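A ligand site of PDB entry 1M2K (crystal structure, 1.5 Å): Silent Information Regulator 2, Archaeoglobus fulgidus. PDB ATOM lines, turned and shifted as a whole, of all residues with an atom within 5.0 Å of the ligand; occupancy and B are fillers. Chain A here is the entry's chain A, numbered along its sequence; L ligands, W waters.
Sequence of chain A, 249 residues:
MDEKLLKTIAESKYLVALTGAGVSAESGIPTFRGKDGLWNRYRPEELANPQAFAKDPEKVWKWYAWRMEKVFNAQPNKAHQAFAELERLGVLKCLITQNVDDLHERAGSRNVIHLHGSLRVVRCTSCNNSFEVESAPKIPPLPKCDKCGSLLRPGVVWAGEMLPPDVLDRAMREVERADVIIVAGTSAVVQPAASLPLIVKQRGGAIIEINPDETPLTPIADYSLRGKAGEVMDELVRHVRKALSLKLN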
ATOM      1  N   GLY A  20       3.699  15.675   8.018  1.00  0.00           N
ATOM      2  CA  GLY A  20       2.784  16.027   9.087  1.00  0.00           C
ATOM      3  C   GLY A  20       2.882  15.003  10.213  1.00  0.00           C
ATOM      4  O   GLY A  20       3.748  14.132  10.195  1.00  0.00           O
ATOM      5  N   ALA A  21       1.990  15.108  11.194  1.00  0.00           N
ATOM      6  CA  ALA A  21       1.988  14.239  12.373  1.00  0.00           C
ATOM      7  C   ALA A  21       1.961  12.734  12.087  1.00  0.00           C
ATOM      8  O   ALA A  21       2.398  11.937  12.923  1.00  0.00           O
ATOM      9  CB  ALA A  21       0.838  14.610  13.285  1.00  0.00           C
ATOM     10  N   GLY A  22       1.435  12.360  10.933  1.00  0.00           N
ATOM     11  CA  GLY A  22       1.368  10.954  10.572  1.00  0.00           C
ATOM     12  C   GLY A  22       2.714  10.269  10.458  1.00  0.00           C
ATOM     13  O   GLY A  22       2.809   9.052  10.658  1.00  0.00           O
ATOM     14  N   VAL A  23       3.762  11.009  10.139  1.00  0.00           N
ATOM     15  CA  VAL A  23       5.070  10.377  10.009  1.00  0.00           C
ATOM     16  C   VAL A  23       5.697  10.059  11.366  1.00  0.00           C
ATOM     17  O   VAL A  23       6.719   9.371  11.427  1.00  0.00           O
ATOM     18  CB  VAL A  23       6.069  11.222   9.167  1.00  0.00           C
ATOM     19  CG1 VAL A  23       5.521  11.422   7.756  1.00  0.00           C
ATOM     20  CG2 VAL A  23       6.348  12.554   9.835  1.00  0.00           C
ATOM     21  N   ALA A  25       3.603   8.959  13.984  1.00  0.00           N
ATOM     22  CA  ALA A  25       2.659   8.061  14.638  1.00  0.00           C
ATOM     23  C   ALA A  25       3.298   6.723  14.983  1.00  0.00           C
ATOM     24  O   ALA A  25       3.044   6.162  16.053  1.00  0.00           O
ATOM     25  CB  ALA A  25       1.444   7.837  13.743  1.00  0.00           C
ATOM     26  N   GLU A  26       4.139   6.227  14.086  1.00  0.00           N
ATOM     27  CA  GLU A  26       4.801   4.950  14.303  1.00  0.00           C
ATOM     28  C   GLU A  26       5.931   5.012  15.318  1.00  0.00           C
ATOM     29  O   GLU A  26       6.647   4.022  15.527  1.00  0.00           O
ATOM     30  CB  GLU A  26       5.275   4.375  12.968  1.00  0.00           C
ATOM     31  CG  GLU A  26       4.110   3.985  12.056  1.00  0.00           C
ATOM     32  CD  GLU A  26       4.520   3.726  10.618  1.00  0.00           C
ATOM     33  OE1 GLU A  26       5.028   2.626  10.317  1.00  0.00           O
ATOM     34  OE2 GLU A  26       4.323   4.638   9.788  1.00  0.00           O
ATOM     35  N   THR A  31      -1.348  11.571  16.689  1.00  0.00           N
ATOM     36  CA  THR A  31      -1.579  12.573  15.666  1.00  0.00           C
ATOM     37  C   THR A  31      -2.602  13.545  16.245  1.00  0.00           C
ATOM     38  O   THR A  31      -3.047  13.367  17.381  1.00  0.00           O
ATOM     39  CB  THR A  31      -2.139  11.967  14.360  1.00  0.00           C
ATOM     40  OG1 THR A  31      -3.398  11.325  14.626  1.00  0.00           O
ATOM     41  CG2 THR A  31      -1.177  10.943  13.787  1.00  0.00           C
ATOM     42  N   PHE A  32      -2.973  14.561  15.477  1.00  0.00           N
ATOM     43  CA  PHE A  32      -3.951  15.542  15.937  1.00  0.00           C
ATOM     44  C   PHE A  32      -5.349  15.171  15.478  1.00  0.00           C
ATOM     45  O   PHE A  32      -6.320  15.329  16.225  1.00  0.00           O
ATOM     46  CB  PHE A  32      -3.599  16.930  15.399  1.00  0.00           C
ATOM     47  CG  PHE A  32      -2.297  17.469  15.921  1.00  0.00           C
ATOM     48  CD1 PHE A  32      -2.226  18.017  17.198  1.00  0.00           C
ATOM     49  CD2 PHE A  32      -1.149  17.412  15.147  1.00  0.00           C
ATOM     50  CE1 PHE A  32      -1.023  18.508  17.695  1.00  0.00           C
ATOM     51  CE2 PHE A  32       0.063  17.904  15.631  1.00  0.00           C
ATOM     52  CZ  PHE A  32       0.121  18.452  16.912  1.00  0.00           C
ATOM     53  N   ARG A  33      -5.446  14.652  14.254  1.00  0.00           N
ATOM     54  CA  ARG A  33      -6.727  14.270  13.673  1.00  0.00           C
ATOM     55  C   ARG A  33      -6.733  12.806  13.236  1.00  0.00           C
ATOM     56  O   ARG A  33      -5.687  12.240  12.899  1.00  0.00           O
ATOM     57  CB  ARG A  33      -7.032  15.186  12.478  1.00  0.00           C
ATOM     58  CG  ARG A  33      -6.896  16.665  12.834  1.00  0.00           C
ATOM     59  CD  ARG A  33      -7.235  17.603  11.693  1.00  0.00           C
ATOM     60  NE  ARG A  33      -7.154  18.997  12.123  1.00  0.00           N
ATOM     61  CZ  ARG A  33      -6.017  19.655  12.358  1.00  0.00           C
ATOM     62  NH1 ARG A  33      -6.051  20.911  12.762  1.00  0.00           N
ATOM     63  NH2 ARG A  33      -4.839  19.058  12.167  1.00  0.00           N
ATOM     64  N   TRP A  39      -6.957  16.007  18.868  1.00  0.00           N
ATOM     65  CA  TRP A  39      -8.084  16.925  18.782  1.00  0.00           C
ATOM     66  C   TRP A  39      -9.439  16.214  18.853  1.00  0.00           C
ATOM     67  O   TRP A  39     -10.480  16.866  18.858  1.00  0.00           O
ATOM     68  CB  TRP A  39      -7.992  17.757  17.499  1.00  0.00           C
ATOM     69  CG  TRP A  39      -6.813  18.723  17.428  1.00  0.00           C
ATOM     70  CD1 TRP A  39      -6.332  19.339  16.312  1.00  0.00           C
ATOM     71  CD2 TRP A  39      -5.994  19.183  18.526  1.00  0.00           C
ATOM     72  NE1 TRP A  39      -5.284  20.163  16.629  1.00  0.00           N
ATOM     73  CE2 TRP A  39      -5.053  20.084  17.979  1.00  0.00           C
ATOM     74  CE3 TRP A  39      -5.974  18.935  19.900  1.00  0.00           C
ATOM     75  CZ2 TRP A  39      -4.097  20.745  18.765  1.00  0.00           C
ATOM     76  CZ3 TRP A  39      -5.025  19.590  20.688  1.00  0.00           C
ATOM     77  CH2 TRP A  39      -4.094  20.478  20.112  1.00  0.00           C
ATOM     78  N   GLN A  98       5.482  20.094   9.524  1.00  0.00           N
ATOM     79  CA  GLN A  98       4.537  20.813  10.375  1.00  0.00           C
ATOM     80  C   GLN A  98       4.716  20.280  11.794  1.00  0.00           C
ATOM     81  O   GLN A  98       4.177  20.849  12.739  1.00  0.00           O
ATOM     82  CB  GLN A  98       3.107  20.537   9.912  1.00  0.00           C
ATOM     83  CG  GLN A  98       2.827  20.986   8.498  1.00  0.00           C
ATOM     84  CD  GLN A  98       1.522  20.447   7.967  1.00  0.00           C
ATOM     85  OE1 GLN A  98       0.452  20.982   8.256  1.00  0.00           O
ATOM     86  NE2 GLN A  98       1.603  19.382   7.183  1.00  0.00           N
ATOM     87  N   ASN A  99       5.483  19.197  11.929  1.00  0.00           N
ATOM     88  CA  ASN A  99       5.703  18.588  13.235  1.00  0.00           C
ATOM     89  C   ASN A  99       6.561  19.414  14.169  1.00  0.00           C
ATOM     90  O   ASN A  99       7.522  20.044  13.764  1.00  0.00           O
ATOM     91  CB  ASN A  99       6.351  17.208  13.082  1.00  0.00           C
ATOM     92  CG  ASN A  99       5.494  16.240  12.295  1.00  0.00           C
ATOM     93  OD1 ASN A  99       4.292  16.458  12.121  1.00  0.00           O
ATOM     94  ND2 ASN A  99       6.096  15.161  11.841  1.00  0.00           N
ATOM     95  N   HIS A 116       5.720  25.062  11.994  1.00  0.00           N
ATOM     96  CA  HIS A 116       4.949  25.382  13.194  1.00  0.00           C
ATOM     97  C   HIS A 116       5.735  25.437  14.506  1.00  0.00           C
ATOM     98  O   HIS A 116       5.172  25.313  15.588  1.00  0.00           O
ATOM     99  CB  HIS A 116       3.798  24.368  13.316  1.00  0.00           C
ATOM    100  CG  HIS A 116       2.891  24.360  12.129  1.00  0.00           C
ATOM    101  ND1 HIS A 116       1.979  23.350  11.904  1.00  0.00           N
ATOM    102  CD2 HIS A 116       2.767  25.226  11.095  1.00  0.00           C
ATOM    103  CE1 HIS A 116       1.325  23.595  10.781  1.00  0.00           C
ATOM    104  NE2 HIS A 116       1.786  24.732  10.265  1.00  0.00           N
ATOM    105  N   GLY A 185       1.917  11.837   5.766  1.00  0.00           N
ATOM    106  CA  GLY A 185       1.356  11.993   7.098  1.00  0.00           C
ATOM    107  C   GLY A 185       0.661  13.282   7.449  1.00  0.00           C
ATOM    108  O   GLY A 185       0.692  13.704   8.603  1.00  0.00           O
ATOM    109  N   THR A 186       0.029  13.938   6.475  1.00  0.00           N
ATOM    110  CA  THR A 186      -0.674  15.166   6.793  1.00  0.00           C
ATOM    111  C   THR A 186      -2.099  15.164   6.242  1.00  0.00           C
ATOM    112  O   THR A 186      -2.369  14.660   5.146  1.00  0.00           O
ATOM    113  CB  THR A 186       0.123  16.409   6.304  1.00  0.00           C
ATOM    114  OG1 THR A 186      -0.582  17.615   6.642  1.00  0.00           O
ATOM    115  CG2 THR A 186       0.364  16.365   4.807  1.00  0.00           C
ATOM    116  N   SER A 187      -3.014  15.727   7.031  1.00  0.00           N
ATOM    117  CA  SER A 187      -4.425  15.778   6.680  1.00  0.00           C
ATOM    118  C   SER A 187      -4.768  16.819   5.621  1.00  0.00           C
ATOM    119  O   SER A 187      -5.899  16.875   5.140  1.00  0.00           O
ATOM    120  CB  SER A 187      -5.251  16.028   7.955  1.00  0.00           C
ATOM    121  OG  SER A 187      -4.774  17.174   8.631  1.00  0.00           O
ATOM    122  N   ALA A 188      -3.785  17.651   5.266  1.00  0.00           N
ATOM    123  CA  ALA A 188      -3.971  18.664   4.240  1.00  0.00           C
ATOM    124  C   ALA A 188      -5.142  19.636   4.445  1.00  0.00           C
ATOM    125  O   ALA A 188      -5.839  19.991   3.491  1.00  0.00           O
ATOM    126  CB  ALA A 188      -4.089  17.996   2.885  1.00  0.00           C
ATOM    127  N   VAL A 190      -4.834  22.230   7.325  1.00  0.00           N
ATOM    128  CA  VAL A 190      -4.265  23.412   7.955  1.00  0.00           C
ATOM    129  C   VAL A 190      -3.422  24.261   6.993  1.00  0.00           C
ATOM    130  O   VAL A 190      -2.526  23.751   6.319  1.00  0.00           O
ATOM    131  CB  VAL A 190      -3.390  23.010   9.175  1.00  0.00           C
ATOM    132  CG1 VAL A 190      -2.716  24.235   9.774  1.00  0.00           C
ATOM    133  CG2 VAL A 190      -4.258  22.330  10.208  1.00  0.00           C
ATOM    134  N   ILE A 210       1.512  10.147   0.668  1.00  0.00           N
ATOM    135  CA  ILE A 210       1.610   8.904   1.443  1.00  0.00           C
ATOM    136  C   ILE A 210       0.754   9.102   2.682  1.00  0.00           C
ATOM    137  O   ILE A 210       1.088   9.887   3.567  1.00  0.00           O
ATOM    138  CB  ILE A 210       3.079   8.604   1.843  1.00  0.00           C
ATOM    139  CG1 ILE A 210       3.921   8.430   0.579  1.00  0.00           C
ATOM    140  CG2 ILE A 210       3.125   7.334   2.695  1.00  0.00           C
ATOM    141  CD1 ILE A 210       5.411   8.221   0.842  1.00  0.00           C
ATOM    142  N   ASN A 211      -0.356   8.364   2.758  1.00  0.00           N
ATOM    143  CA  ASN A 211      -1.288   8.531   3.861  1.00  0.00           C
ATOM    144  C   ASN A 211      -2.287   7.361   3.861  1.00  0.00           C
ATOM    145  O   ASN A 211      -2.777   6.973   2.800  1.00  0.00           O
ATOM    146  CB  ASN A 211      -2.029   9.856   3.662  1.00  0.00           C
ATOM    147  CG  ASN A 211      -2.742  10.334   4.896  1.00  0.00           C
ATOM    148  OD1 ASN A 211      -3.489   9.591   5.530  1.00  0.00           O
ATOM    149  ND2 ASN A 211      -2.523  11.599   5.252  1.00  0.00           N
ATOM    150  N   PRO A 212      -2.588   6.793   5.040  1.00  0.00           N
ATOM    151  CA  PRO A 212      -3.532   5.672   5.110  1.00  0.00           C
ATOM    152  C   PRO A 212      -4.966   6.113   4.814  1.00  0.00           C
ATOM    153  O   PRO A 212      -5.869   5.290   4.693  1.00  0.00           O
ATOM    154  CB  PRO A 212      -3.394   5.177   6.555  1.00  0.00           C
ATOM    155  CG  PRO A 212      -2.016   5.610   6.941  1.00  0.00           C
ATOM    156  CD  PRO A 212      -1.911   6.978   6.332  1.00  0.00           C
ATOM    157  N   ASP A 213      -5.166   7.427   4.707  1.00  0.00           N
ATOM    158  CA  ASP A 213      -6.498   7.979   4.450  1.00  0.00           C
ATOM    159  C   ASP A 213      -6.419   8.928   3.263  1.00  0.00           C
ATOM    160  O   ASP A 213      -5.338   9.404   2.894  1.00  0.00           O
ATOM    161  CB  ASP A 213      -7.000   8.738   5.680  1.00  0.00           C
ATOM    162  CG  ASP A 213      -8.467   9.094   5.598  1.00  0.00           C
ATOM    163  OD1 ASP A 213      -8.933   9.902   6.442  1.00  0.00           O
ATOM    164  OD2 ASP A 213      -9.174   8.580   4.702  1.00  0.00           O
ATOM    165  N   THR A 215      -7.225  12.544   1.501  1.00  0.00           N
ATOM    166  CA  THR A 215      -7.248  13.900   2.035  1.00  0.00           C
ATOM    167  C   THR A 215      -7.705  14.839   0.920  1.00  0.00           C
ATOM    168  O   THR A 215      -7.936  14.404  -0.204  1.00  0.00           O
ATOM    169  CB  THR A 215      -5.836  14.356   2.474  1.00  0.00           C
ATOM    170  OG1 THR A 215      -5.077  14.730   1.327  1.00  0.00           O
ATOM    171  CG2 THR A 215      -5.112  13.228   3.207  1.00  0.00           C
ATOM    172  N   GLY A 227      -1.100   3.891   2.635  1.00  0.00           N
ATOM    173  CA  GLY A 227      -0.443   3.062   3.631  1.00  0.00           C
ATOM    174  C   GLY A 227       0.314   3.878   4.669  1.00  0.00           C
ATOM    175  O   GLY A 227       0.271   5.103   4.653  1.00  0.00           O
ATOM    176  N   LYS A 228       0.994   3.179   5.572  1.00  0.00           N
ATOM    177  CA  LYS A 228       1.767   3.829   6.625  1.00  0.00           C
ATOM    178  C   LYS A 228       3.107   4.335   6.083  1.00  0.00           C
ATOM    179  O   LYS A 228       3.762   3.650   5.293  1.00  0.00           O
ATOM    180  CB  LYS A 228       2.020   2.869   7.781  1.00  0.00           C
ATOM    181  CG  LYS A 228       0.767   2.390   8.498  1.00  0.00           C
ATOM    182  CD  LYS A 228       1.112   1.445   9.636  1.00  0.00           C
ATOM    183  CE  LYS A 228      -0.135   0.924  10.338  1.00  0.00           C
ATOM    184  NZ  LYS A 228      -0.897   2.013  11.011  1.00  0.00           N
ATOM    185  N   ALA A 229       3.504   5.519   6.524  1.00  0.00           N
ATOM    186  CA  ALA A 229       4.754   6.135   6.070  1.00  0.00           C
ATOM    187  C   ALA A 229       5.979   5.264   6.338  1.00  0.00           C
ATOM    188  O   ALA A 229       6.908   5.226   5.529  1.00  0.00           O
ATOM    189  CB  ALA A 229       4.939   7.504   6.718  1.00  0.00           C
ATOM    190  N   GLY A 230       5.985   4.587   7.476  1.00  0.00           N
ATOM    191  CA  GLY A 230       7.116   3.750   7.818  1.00  0.00           C
ATOM    192  C   GLY A 230       7.357   2.654   6.794  1.00  0.00           C
ATOM    193  O   GLY A 230       8.469   2.510   6.276  1.00  0.00           O
HETATM  194  N1  LIG L   1       1.785   7.079   8.204  1.00  0.00           N
HETATM  195  C1  LIG L   1       1.414   8.161   7.398  1.00  0.00           C
HETATM  196  N2  LIG L   1       0.298   8.925   7.729  1.00  0.00           N
HETATM  197  C2  LIG L   1      -0.443   8.600   8.853  1.00  0.00           C
HETATM  198  C3  LIG L   1      -0.096   7.513   9.655  1.00  0.00           C
HETATM  199  C4  LIG L   1       1.045   6.726   9.336  1.00  0.00           C
HETATM  200  N3  LIG L   1       1.427   5.681  10.098  1.00  0.00           N
HETATM  201  N4  LIG L   1      -0.973   7.439  10.650  1.00  0.00           N
HETATM  202  C5  LIG L   1      -1.858   8.456  10.464  1.00  0.00           C
HETATM  203  N5  LIG L   1      -1.582   9.260   9.320  1.00  0.00           N
HETATM  204  C6  LIG L   1      -2.158  10.406   8.699  1.00  0.00           C
HETATM  205  C7  LIG L   1      -3.563  10.543   8.950  1.00  0.00           C
HETATM  206  O1  LIG L   1      -4.351   9.781   8.199  1.00  0.00           O
HETATM  207  C8  LIG L   1      -3.758  11.956   8.838  1.00  0.00           C
HETATM  208  O2  LIG L   1      -4.201  12.337   7.628  1.00  0.00           O
HETATM  209  O3  LIG L   1      -1.623  11.510   9.239  1.00  0.00           O
HETATM  210  C9  LIG L   1      -2.466  12.545   9.062  1.00  0.00           C
HETATM  211  C10 LIG L   1      -2.327  13.426  10.225  1.00  0.00           C
HETATM  212  O4  LIG L   1      -3.156  14.469  10.139  1.00  0.00           O
HETATM  213  P1  LIG L   1      -3.101  15.538  11.373  1.00  0.00           P
HETATM  214  O5  LIG L   1      -3.340  14.820  12.753  1.00  0.00           O
HETATM  215  O6  LIG L   1      -4.186  16.646  11.099  1.00  0.00           O
HETATM  216  O7  LIG L   1      -1.606  16.167  11.452  1.00  0.00           O
HETATM  217  P2  LIG L   1      -1.104  17.398  10.509  1.00  0.00           P
HETATM  218  O8  LIG L   1      -1.544  17.281   8.990  1.00  0.00           O
HETATM  219  O9  LIG L   1       0.465  17.443  10.640  1.00  0.00           O
HETATM  220  O10 LIG L   1      -1.651  18.695  11.371  1.00  0.00           O
HETATM  221  C11 LIG L   1      -1.473  20.031  10.884  1.00  0.00           C
HETATM  222  O11 LIG L   1      -2.458  20.888  12.840  1.00  0.00           O
HETATM  223  O12 LIG L   1      -3.192  21.461  14.666  1.00  0.00           O
HETATM  224  C12 LIG L   1      -2.306  20.758  14.023  1.00  0.00           C
HETATM  225  O13 LIG L   1      -0.823  22.208  14.500  1.00  0.00           O
HETATM  226  C13 LIG L   1      -1.041  21.100  14.280  1.00  0.00           C
HETATM  227  O14 LIG L   1       0.888  20.766  13.052  1.00  0.00           O
HETATM  228  C14 LIG L   1      -0.403  20.501  13.186  1.00  0.00           C
HETATM  229  C15 LIG L   1      -1.216  20.802  12.066  1.00  0.00           C
HETATM  230  O   HOH W   1      -3.617  19.625   7.810  1.00  0.00           O
HETATM  231  O   HOH W   2      -6.818  11.982   7.563  1.00  0.00           O
HETATM  232  O   HOH W   3       0.390   4.319  12.376  1.00  0.00           O
HETATM  233  O   HOH W   4       2.180  18.219  12.572  1.00  0.00           O
HETATM  234  O   HOH W   5       2.676  19.855  15.094  1.00  0.00           O
HETATM  235  O   HOH W   6      -4.794   9.993  11.851  1.00  0.00           O
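O6 of the ligand is in hydrogen-bond range of OG of Ser 187. O5 of the ligand lies within hydrogen-bond range of N of Phe 32, at 2.8 Å. An oxygen (O14) of the ligand lies within hydrogen-bond range of the backbone carbonyl oxygen (O) of Gln 98, 3.3 Å away. An oxygen (O12) of the ligand sits at hydrogen-bond distance from the indole nitrogen of Trp 39. The backbone NH (N) of Ala 229 is in hydrogen-bond range of a nitrogen (N1) of the ligand, 2.9 Å away. A ring nitrogen (ND1) of His 116 is in hydrogen-bond range of an oxygen (O14) of the ligand (3.0 Å). The side-chain carboxylate (OE2) of Glu 26 is in hydrogen-bond range of a nitrogen (N3) of the ligand (3.1 Å). OD1 of Asn 211 is in hydrogen-bond range of O1 of the ligand, at 2.8 Å. NH2 of Arg 33 sits at hydrogen-bond distance from O6 of the ligand, at 2.7 Å. The backbone NH (N) of Ser 187 lies within hydrogen-bond range of an oxygen (O8) of the ligand, 2.9 Å away. N of Ala 21 is in hydrogen-bond range of O9 of the ligand, at 2.8 Å. The backbone NH (N) of Arg 33 sits at hydrogen-bond distance from an oxygen (O5) of the ligand (2.6 Å). The side-chain hydroxyl of Thr 186 lies within hydrogen-bond range of an oxygen (O8) of the ligand (2.6 Å).
OG1 of Thr 186 sits close to N of Ala 188 (3.5 Å). O of Arg 33 lies within hydrogen-bond range of OG1 of Thr 31 (3.0 Å). NE2 of Gln 98 is in hydrogen-bond range of OG1 of Thr 186. OD1 of Asn 211 sits at hydrogen-bond distance from N of Asp 213 (2.9 Å). N of Gly 22 sits at hydrogen-bond distance from O of Gly 185, 2.8 Å away. N of Ala 229 is in hydrogen-bond range of OE2 of Glu 26 (3.5 Å). The backbone carbonyl oxygen of Ile 210 sits at hydrogen-bond distance from the backbone NH of Gly 185, 3.1 Å away. OE2 of Glu 26 sits at hydrogen-bond distance from N of Gly 230, 2.8 Å away.
A nitrogen (N1) of the ligand sits close to the backbone carbonyl oxygen (O) of Gly 22 (3.3 Å). O of Gly 185 lies close to O3 of the ligand (3.3 Å). Residues that only touch the ligand: Gly 20, Pro 212, Thr 31, Val 190, Lys 228, Asp 213 and Ala 25. Hydrophobic or aromatic side chains that line the ligand: Ala 21, Ala 25, Phe 32, His 116, Val 190, Pro 212 and Ala 229. Within 4 Å of the ligand: Gly 20, Ala 21, Gly 22, Ala 25, Glu 26, Thr 31, Phe 32, Arg 33, Trp 39, Gln 98, His 116, Gly 185, Thr 186, Ser 187, Val 190, Asn 211, Pro 212, Asp 213, Lys 228 and Ala 229. The nearest printed residue that does not touch the ligand is Ile 210 (4.2 Å).
Water W2 lies within hydrogen-bond range of an oxygen (O2) of the ligand (2.6 Å) and the side-chain carboxylate (OD1) of Asp 213 (3.2 Å). Water W4 lies within hydrogen-bond range of an oxygen (O9) of the ligand (2.7 Å), the side-chain amide oxygen of Asn 99 (2.8 Å), the backbone carbonyl oxygen of Gln 98 (3.3 Å) and the backbone NH of Ala 21 (3.4 Å). Water W3 bridges N3 of the ligand and NZ of Lys 228. Water W5 lies within hydrogen-bond range of an oxygen (O14) of the ligand and the backbone carbonyl oxygen of Gln 98. Water W6 bridges O of Arg 33 (2.6 Å) and OG1 of Thr 31 (3.4 Å). Water W1 lies within hydrogen-bond range of OG of Ser 187, N of Val 190, N of Ala 188 and O8 of the ligand.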
